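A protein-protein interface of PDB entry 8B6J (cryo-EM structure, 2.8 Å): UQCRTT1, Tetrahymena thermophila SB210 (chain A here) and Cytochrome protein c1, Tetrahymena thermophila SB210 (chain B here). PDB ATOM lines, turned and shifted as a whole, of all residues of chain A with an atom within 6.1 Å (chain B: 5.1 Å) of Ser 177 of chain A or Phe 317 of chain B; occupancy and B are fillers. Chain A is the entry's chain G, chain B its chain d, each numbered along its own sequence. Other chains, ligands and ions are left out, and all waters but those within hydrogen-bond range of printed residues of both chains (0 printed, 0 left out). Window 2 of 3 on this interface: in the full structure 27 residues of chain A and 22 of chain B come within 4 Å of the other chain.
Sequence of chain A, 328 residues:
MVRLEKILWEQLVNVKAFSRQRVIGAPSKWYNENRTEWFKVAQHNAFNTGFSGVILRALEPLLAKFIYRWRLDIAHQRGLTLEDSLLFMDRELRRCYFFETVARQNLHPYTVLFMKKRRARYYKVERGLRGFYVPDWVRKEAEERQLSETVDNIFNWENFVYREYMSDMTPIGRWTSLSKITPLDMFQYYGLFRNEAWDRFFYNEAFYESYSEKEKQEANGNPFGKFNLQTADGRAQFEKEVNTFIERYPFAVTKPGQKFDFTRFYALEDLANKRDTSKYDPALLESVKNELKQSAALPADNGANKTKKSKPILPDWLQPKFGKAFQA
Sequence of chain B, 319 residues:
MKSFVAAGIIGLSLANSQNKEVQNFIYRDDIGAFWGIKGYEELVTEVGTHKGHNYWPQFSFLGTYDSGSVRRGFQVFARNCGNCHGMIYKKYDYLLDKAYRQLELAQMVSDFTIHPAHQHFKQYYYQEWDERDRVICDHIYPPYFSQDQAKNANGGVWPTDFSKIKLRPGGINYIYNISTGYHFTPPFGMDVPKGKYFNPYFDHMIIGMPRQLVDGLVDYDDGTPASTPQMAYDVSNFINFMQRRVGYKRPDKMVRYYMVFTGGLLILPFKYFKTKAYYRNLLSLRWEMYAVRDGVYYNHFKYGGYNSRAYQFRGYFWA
The backbone carbonyl oxygen (O) of Arg 174 of chain A sits at hydrogen-bond distance from the backbone NH (N) of Tyr 190 of chain A (2.9 Å).
Ser 177 of chain A touches just these residues of chain B: Gln 312 (3.5 Å) and Phe 317 (3.4 Å). Of the printed residues of chain A, Tyr 316 of chain B touches Arg 174. Of the printed residues of chain B, Arg 174 of chain A touches Tyr 316 (3.5 Å) and Phe 317 (3.6 Å). Printed residues of chain A within 4 Å of Gln 312 of chain B: Ser 177 (3.5 Å) and Leu 178 (2.9 Å). Printed residues of chain B within 4 Å of Leu 178 of chain A: Gln 312 (2.9 Å). Gln 188 of chain A touches none of the printed residues of chain B. The nearest residue of chain B that does not touch Ser 177 of chain A is Tyr 316 of chain B (4.1 Å).
CD1 of Tyr 316 of chain B touches CD of Arg 174 of chain A, 3.5 Å away. Arg 174 of chain A touches Phe 317 of chain B. CB of Ser 177 of chain A touches O of Gln 312 of chain B, at 3.5 Å. Ser 177 of chain A touches Phe 317 of chain B. OE1 of Gln 312 of chain B touches CD2 of Leu 178 of chain A, at 2.9 Å.
Printed residues of chain B that touch a printed residue of chain A: Gln 312, Tyr 316 and Phe 317. Hydrophobic or aromatic side chains of chain B that line the printed part of chain A: Tyr 316 and Phe 317. Among the printed residues, no Asp or Glu carboxylate lies within 4 Å of a Lys or Arg side-chain nitrogen of the other chain.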
ATOM      1  N   ARG A 174     -18.607  25.118 -23.665  1.00  0.00           N
ATOM      2  CA  ARG A 174     -19.365  24.590 -24.785  1.00  0.00           C
ATOM      3  C   ARG A 174     -18.856  25.181 -26.092  1.00  0.00           C
ATOM      4  O   ARG A 174     -18.306  26.285 -26.121  1.00  0.00           O
ATOM      5  CB  ARG A 174     -20.857  24.897 -24.601  1.00  0.00           C
ATOM      6  CG  ARG A 174     -21.770  24.237 -25.604  1.00  0.00           C
ATOM      7  CD  ARG A 174     -23.230  24.508 -25.286  1.00  0.00           C
ATOM      8  NE  ARG A 174     -23.515  25.928 -25.117  1.00  0.00           N
ATOM      9  CZ  ARG A 174     -23.803  26.761 -26.107  1.00  0.00           C
ATOM     10  NH1 ARG A 174     -23.826  26.360 -27.367  1.00  0.00           N
ATOM     11  NH2 ARG A 174     -24.073  28.032 -25.826  1.00  0.00           N
ATOM     12  N   TRP A 175     -19.040  24.428 -27.171  1.00  0.00           N
ATOM     13  CA  TRP A 175     -18.779  24.883 -28.525  1.00  0.00           C
ATOM     14  C   TRP A 175     -20.104  25.262 -29.185  1.00  0.00           C
ATOM     15  O   TRP A 175     -21.153  25.317 -28.541  1.00  0.00           O
ATOM     16  CB  TRP A 175     -18.038  23.803 -29.320  1.00  0.00           C
ATOM     17  CG  TRP A 175     -16.573  23.707 -29.015  1.00  0.00           C
ATOM     18  CD1 TRP A 175     -15.950  22.734 -28.294  1.00  0.00           C
ATOM     19  CD2 TRP A 175     -15.549  24.616 -29.433  1.00  0.00           C
ATOM     20  NE1 TRP A 175     -14.601  22.982 -28.234  1.00  0.00           N
ATOM     21  CE2 TRP A 175     -14.330  24.132 -28.924  1.00  0.00           C
ATOM     22  CE3 TRP A 175     -15.544  25.794 -30.185  1.00  0.00           C
ATOM     23  CZ2 TRP A 175     -13.120  24.784 -29.143  1.00  0.00           C
ATOM     24  CZ3 TRP A 175     -14.341  26.439 -30.401  1.00  0.00           C
ATOM     25  CH2 TRP A 175     -13.148  25.933 -29.884  1.00  0.00           C
ATOM     26  N   THR A 176     -20.065  25.540 -30.483  1.00  0.00           N
ATOM     27  CA  THR A 176     -21.293  25.816 -31.217  1.00  0.00           C
ATOM     28  C   THR A 176     -22.258  24.647 -31.077  1.00  0.00           C
ATOM     29  O   THR A 176     -21.962  23.531 -31.513  1.00  0.00           O
ATOM     30  CB  THR A 176     -20.981  26.066 -32.688  1.00  0.00           C
ATOM     31  OG1 THR A 176     -19.934  27.037 -32.800  1.00  0.00           O
ATOM     32  CG2 THR A 176     -22.218  26.571 -33.417  1.00  0.00           C
ATOM     33  N   SER A 177     -23.417  24.903 -30.467  1.00  0.00           N
ATOM     34  CA  SER A 177     -24.441  23.867 -30.385  1.00  0.00           C
ATOM     35  C   SER A 177     -24.924  23.475 -31.773  1.00  0.00           C
ATOM     36  O   SER A 177     -25.166  22.294 -32.045  1.00  0.00           O
ATOM     37  CB  SER A 177     -25.611  24.350 -29.529  1.00  0.00           C
ATOM     38  OG  SER A 177     -26.244  25.470 -30.121  1.00  0.00           O
ATOM     39  N   LEU A 178     -25.070  24.453 -32.662  1.00  0.00           N
ATOM     40  CA  LEU A 178     -25.455  24.167 -34.035  1.00  0.00           C
ATOM     41  C   LEU A 178     -24.375  23.339 -34.719  1.00  0.00           C
ATOM     42  O   LEU A 178     -23.181  23.486 -34.447  1.00  0.00           O
ATOM     43  CB  LEU A 178     -25.677  25.465 -34.809  1.00  0.00           C
ATOM     44  CG  LEU A 178     -26.495  26.560 -34.123  1.00  0.00           C
ATOM     45  CD1 LEU A 178     -26.531  27.801 -34.992  1.00  0.00           C
ATOM     46  CD2 LEU A 178     -27.899  26.076 -33.820  1.00  0.00           C
ATOM     47  N   SER A 179     -24.806  22.458 -35.621  1.00  0.00           N
ATOM     48  CA  SER A 179     -23.892  21.621 -36.390  1.00  0.00           C
ATOM     49  C   SER A 179     -23.536  22.234 -37.736  1.00  0.00           C
ATOM     50  O   SER A 179     -23.257  21.502 -38.695  1.00  0.00           O
ATOM     51  CB  SER A 179     -24.498  20.232 -36.582  1.00  0.00           C
ATOM     52  OG  SER A 179     -24.725  19.603 -35.333  1.00  0.00           O
ATOM     53  N   GLN A 188     -17.326  29.122 -32.625  1.00  0.00           N
ATOM     54  CA  GLN A 188     -17.848  29.872 -31.491  1.00  0.00           C
ATOM     55  C   GLN A 188     -17.472  29.175 -30.191  1.00  0.00           C
ATOM     56  O   GLN A 188     -17.637  27.960 -30.052  1.00  0.00           O
ATOM     57  CB  GLN A 188     -19.364  30.017 -31.600  1.00  0.00           C
ATOM     58  CG  GLN A 188     -19.813  30.833 -32.793  1.00  0.00           C
ATOM     59  CD  GLN A 188     -21.311  31.034 -32.826  1.00  0.00           C
ATOM     60  OE1 GLN A 188     -22.032  30.553 -31.954  1.00  0.00           O
ATOM     61  NE2 GLN A 188     -21.788  31.751 -33.835  1.00  0.00           N
ATOM     62  N   TYR A 190     -17.921  29.158 -26.099  1.00  0.00           N
ATOM     63  CA  TYR A 190     -18.733  29.569 -24.961  1.00  0.00           C
ATOM     64  C   TYR A 190     -18.060  29.119 -23.675  1.00  0.00           C
ATOM     65  O   TYR A 190     -17.607  27.974 -23.573  1.00  0.00           O
ATOM     66  CB  TYR A 190     -20.141  28.984 -25.056  1.00  0.00           C
ATOM     67  CG  TYR A 190     -20.886  29.405 -26.300  1.00  0.00           C
ATOM     68  CD1 TYR A 190     -20.753  28.696 -27.483  1.00  0.00           C
ATOM     69  CD2 TYR A 190     -21.721  30.512 -26.290  1.00  0.00           C
ATOM     70  CE1 TYR A 190     -21.429  29.077 -28.620  1.00  0.00           C
ATOM     71  CE2 TYR A 190     -22.402  30.899 -27.424  1.00  0.00           C
ATOM     72  CZ  TYR A 190     -22.252  30.178 -28.586  1.00  0.00           C
ATOM     73  OH  TYR A 190     -22.929  30.558 -29.721  1.00  0.00           O
ATOM     74  N   GLN B 312     -29.585  19.544 -31.554  1.00  0.00           N
ATOM     75  CA  GLN B 312     -28.832  20.751 -31.243  1.00  0.00           C
ATOM     76  C   GLN B 312     -28.967  21.169 -29.787  1.00  0.00           C
ATOM     77  O   GLN B 312     -28.175  21.997 -29.325  1.00  0.00           O
ATOM     78  CB  GLN B 312     -29.285  21.901 -32.144  1.00  0.00           C
ATOM     79  CG  GLN B 312     -29.039  21.664 -33.619  1.00  0.00           C
ATOM     80  CD  GLN B 312     -29.372  22.872 -34.463  1.00  0.00           C
ATOM     81  OE1 GLN B 312     -29.840  23.888 -33.953  1.00  0.00           O
ATOM     82  NE2 GLN B 312     -29.130  22.771 -35.762  1.00  0.00           N
ATOM     83  N   PHE B 313     -29.939  20.624 -29.060  1.00  0.00           N
ATOM     84  CA  PHE B 313     -30.114  20.930 -27.647  1.00  0.00           C
ATOM     85  C   PHE B 313     -29.591  19.832 -26.736  1.00  0.00           C
ATOM     86  O   PHE B 313     -29.174  20.123 -25.611  1.00  0.00           O
ATOM     87  CB  PHE B 313     -31.596  21.164 -27.331  1.00  0.00           C
ATOM     88  CG  PHE B 313     -32.261  22.172 -28.225  1.00  0.00           C
ATOM     89  CD1 PHE B 313     -31.546  23.226 -28.765  1.00  0.00           C
ATOM     90  CD2 PHE B 313     -33.606  22.061 -28.528  1.00  0.00           C
ATOM     91  CE1 PHE B 313     -32.161  24.148 -29.588  1.00  0.00           C
ATOM     92  CE2 PHE B 313     -34.223  22.980 -29.350  1.00  0.00           C
ATOM     93  CZ  PHE B 313     -33.500  24.025 -29.881  1.00  0.00           C
ATOM     94  N   GLY B 315     -27.348  17.499 -24.759  1.00  0.00           N
ATOM     95  CA  GLY B 315     -25.970  17.569 -24.328  1.00  0.00           C
ATOM     96  C   GLY B 315     -25.382  18.960 -24.279  1.00  0.00           C
ATOM     97  O   GLY B 315     -24.190  19.098 -23.977  1.00  0.00           O
ATOM     98  N   TYR B 316     -26.167  19.992 -24.559  1.00  0.00           N
ATOM     99  CA  TYR B 316     -25.664  21.361 -24.599  1.00  0.00           C
ATOM    100  C   TYR B 316     -26.416  22.312 -23.680  1.00  0.00           C
ATOM    101  O   TYR B 316     -25.788  23.168 -23.051  1.00  0.00           O
ATOM    102  CB  TYR B 316     -25.728  21.890 -26.042  1.00  0.00           C
ATOM    103  CG  TYR B 316     -24.802  21.182 -27.005  1.00  0.00           C
ATOM    104  CD1 TYR B 316     -23.470  21.554 -27.118  1.00  0.00           C
ATOM    105  CD2 TYR B 316     -25.262  20.149 -27.808  1.00  0.00           C
ATOM    106  CE1 TYR B 316     -22.622  20.912 -27.998  1.00  0.00           C
ATOM    107  CE2 TYR B 316     -24.421  19.502 -28.691  1.00  0.00           C
ATOM    108  CZ  TYR B 316     -23.102  19.888 -28.781  1.00  0.00           C
ATOM    109  OH  TYR B 316     -22.260  19.246 -29.659  1.00  0.00           O
ATOM    110  N   PHE B 317     -27.736  22.182 -23.575  1.00  0.00           N
ATOM    111  CA  PHE B 317     -28.572  23.168 -22.903  1.00  0.00           C
ATOM    112  C   PHE B 317     -29.297  22.557 -21.713  1.00  0.00           C
ATOM    113  O   PHE B 317     -29.589  21.360 -21.687  1.00  0.00           O
ATOM    114  CB  PHE B 317     -29.620  23.755 -23.858  1.00  0.00           C
ATOM    115  CG  PHE B 317     -29.046  24.503 -25.025  1.00  0.00           C
ATOM    116  CD1 PHE B 317     -27.786  25.071 -24.962  1.00  0.00           C
ATOM    117  CD2 PHE B 317     -29.778  24.644 -26.187  1.00  0.00           C
ATOM    118  CE1 PHE B 317     -27.270  25.759 -26.040  1.00  0.00           C
ATOM    119  CE2 PHE B 317     -29.268  25.330 -27.265  1.00  0.00           C
ATOM    120  CZ  PHE B 317     -28.013  25.889 -27.192  1.00  0.00           C
ATOM    121  N   TRP B 318     -29.580  23.404 -20.722  1.00  0.00           N
ATOM    122  CA  TRP B 318     -30.499  23.091 -19.629  1.00  0.00           C
ATOM    123  C   TRP B 318     -30.100  21.786 -18.932  1.00  0.00           C
ATOM    124  O   TRP B 318     -30.828  20.792 -18.928  1.00  0.00           O
ATOM    125  CB  TRP B 318     -31.943  23.027 -20.142  1.00  0.00           C
ATOM    126  CG  TRP B 318     -32.278  24.108 -21.127  1.00  0.00           C
ATOM    127  CD1 TRP B 318     -32.173  25.454 -20.938  1.00  0.00           C
ATOM    128  CD2 TRP B 318     -32.785  23.928 -22.454  1.00  0.00           C
ATOM    129  NE1 TRP B 318     -32.575  26.123 -22.068  1.00  0.00           N
ATOM    130  CE2 TRP B 318     -32.956  25.209 -23.013  1.00  0.00           C
ATOM    131  CE3 TRP B 318     -33.107  22.808 -23.226  1.00  0.00           C
ATOM    132  CZ2 TRP B 318     -33.436  25.399 -24.306  1.00  0.00           C
ATOM    133  CZ3 TRP B 318     -33.581  23.000 -24.507  1.00  0.00           C
ATOM    134  CH2 TRP B 318     -33.741  24.284 -25.034  1.00  0.00           C
ATOM    135  N   ALA B 319     -28.911  21.822 -18.347  1.00  0.00           N
ATOM    136  CA  ALA B 319     -28.422  20.712 -17.540  1.00  0.00           C
ATOM    137  C   ALA B 319     -27.198  21.155 -16.756  1.00  0.00           C
ATOM    138  O   ALA B 319     -26.789  20.512 -15.790  1.00  0.00           O
ATOM    139  CB  ALA B 319     -28.093  19.519 -18.413  1.00  0.00           C
ATOM    140  OXT ALA B 319     -26.592  22.178 -17.072  1.00  0.00           O
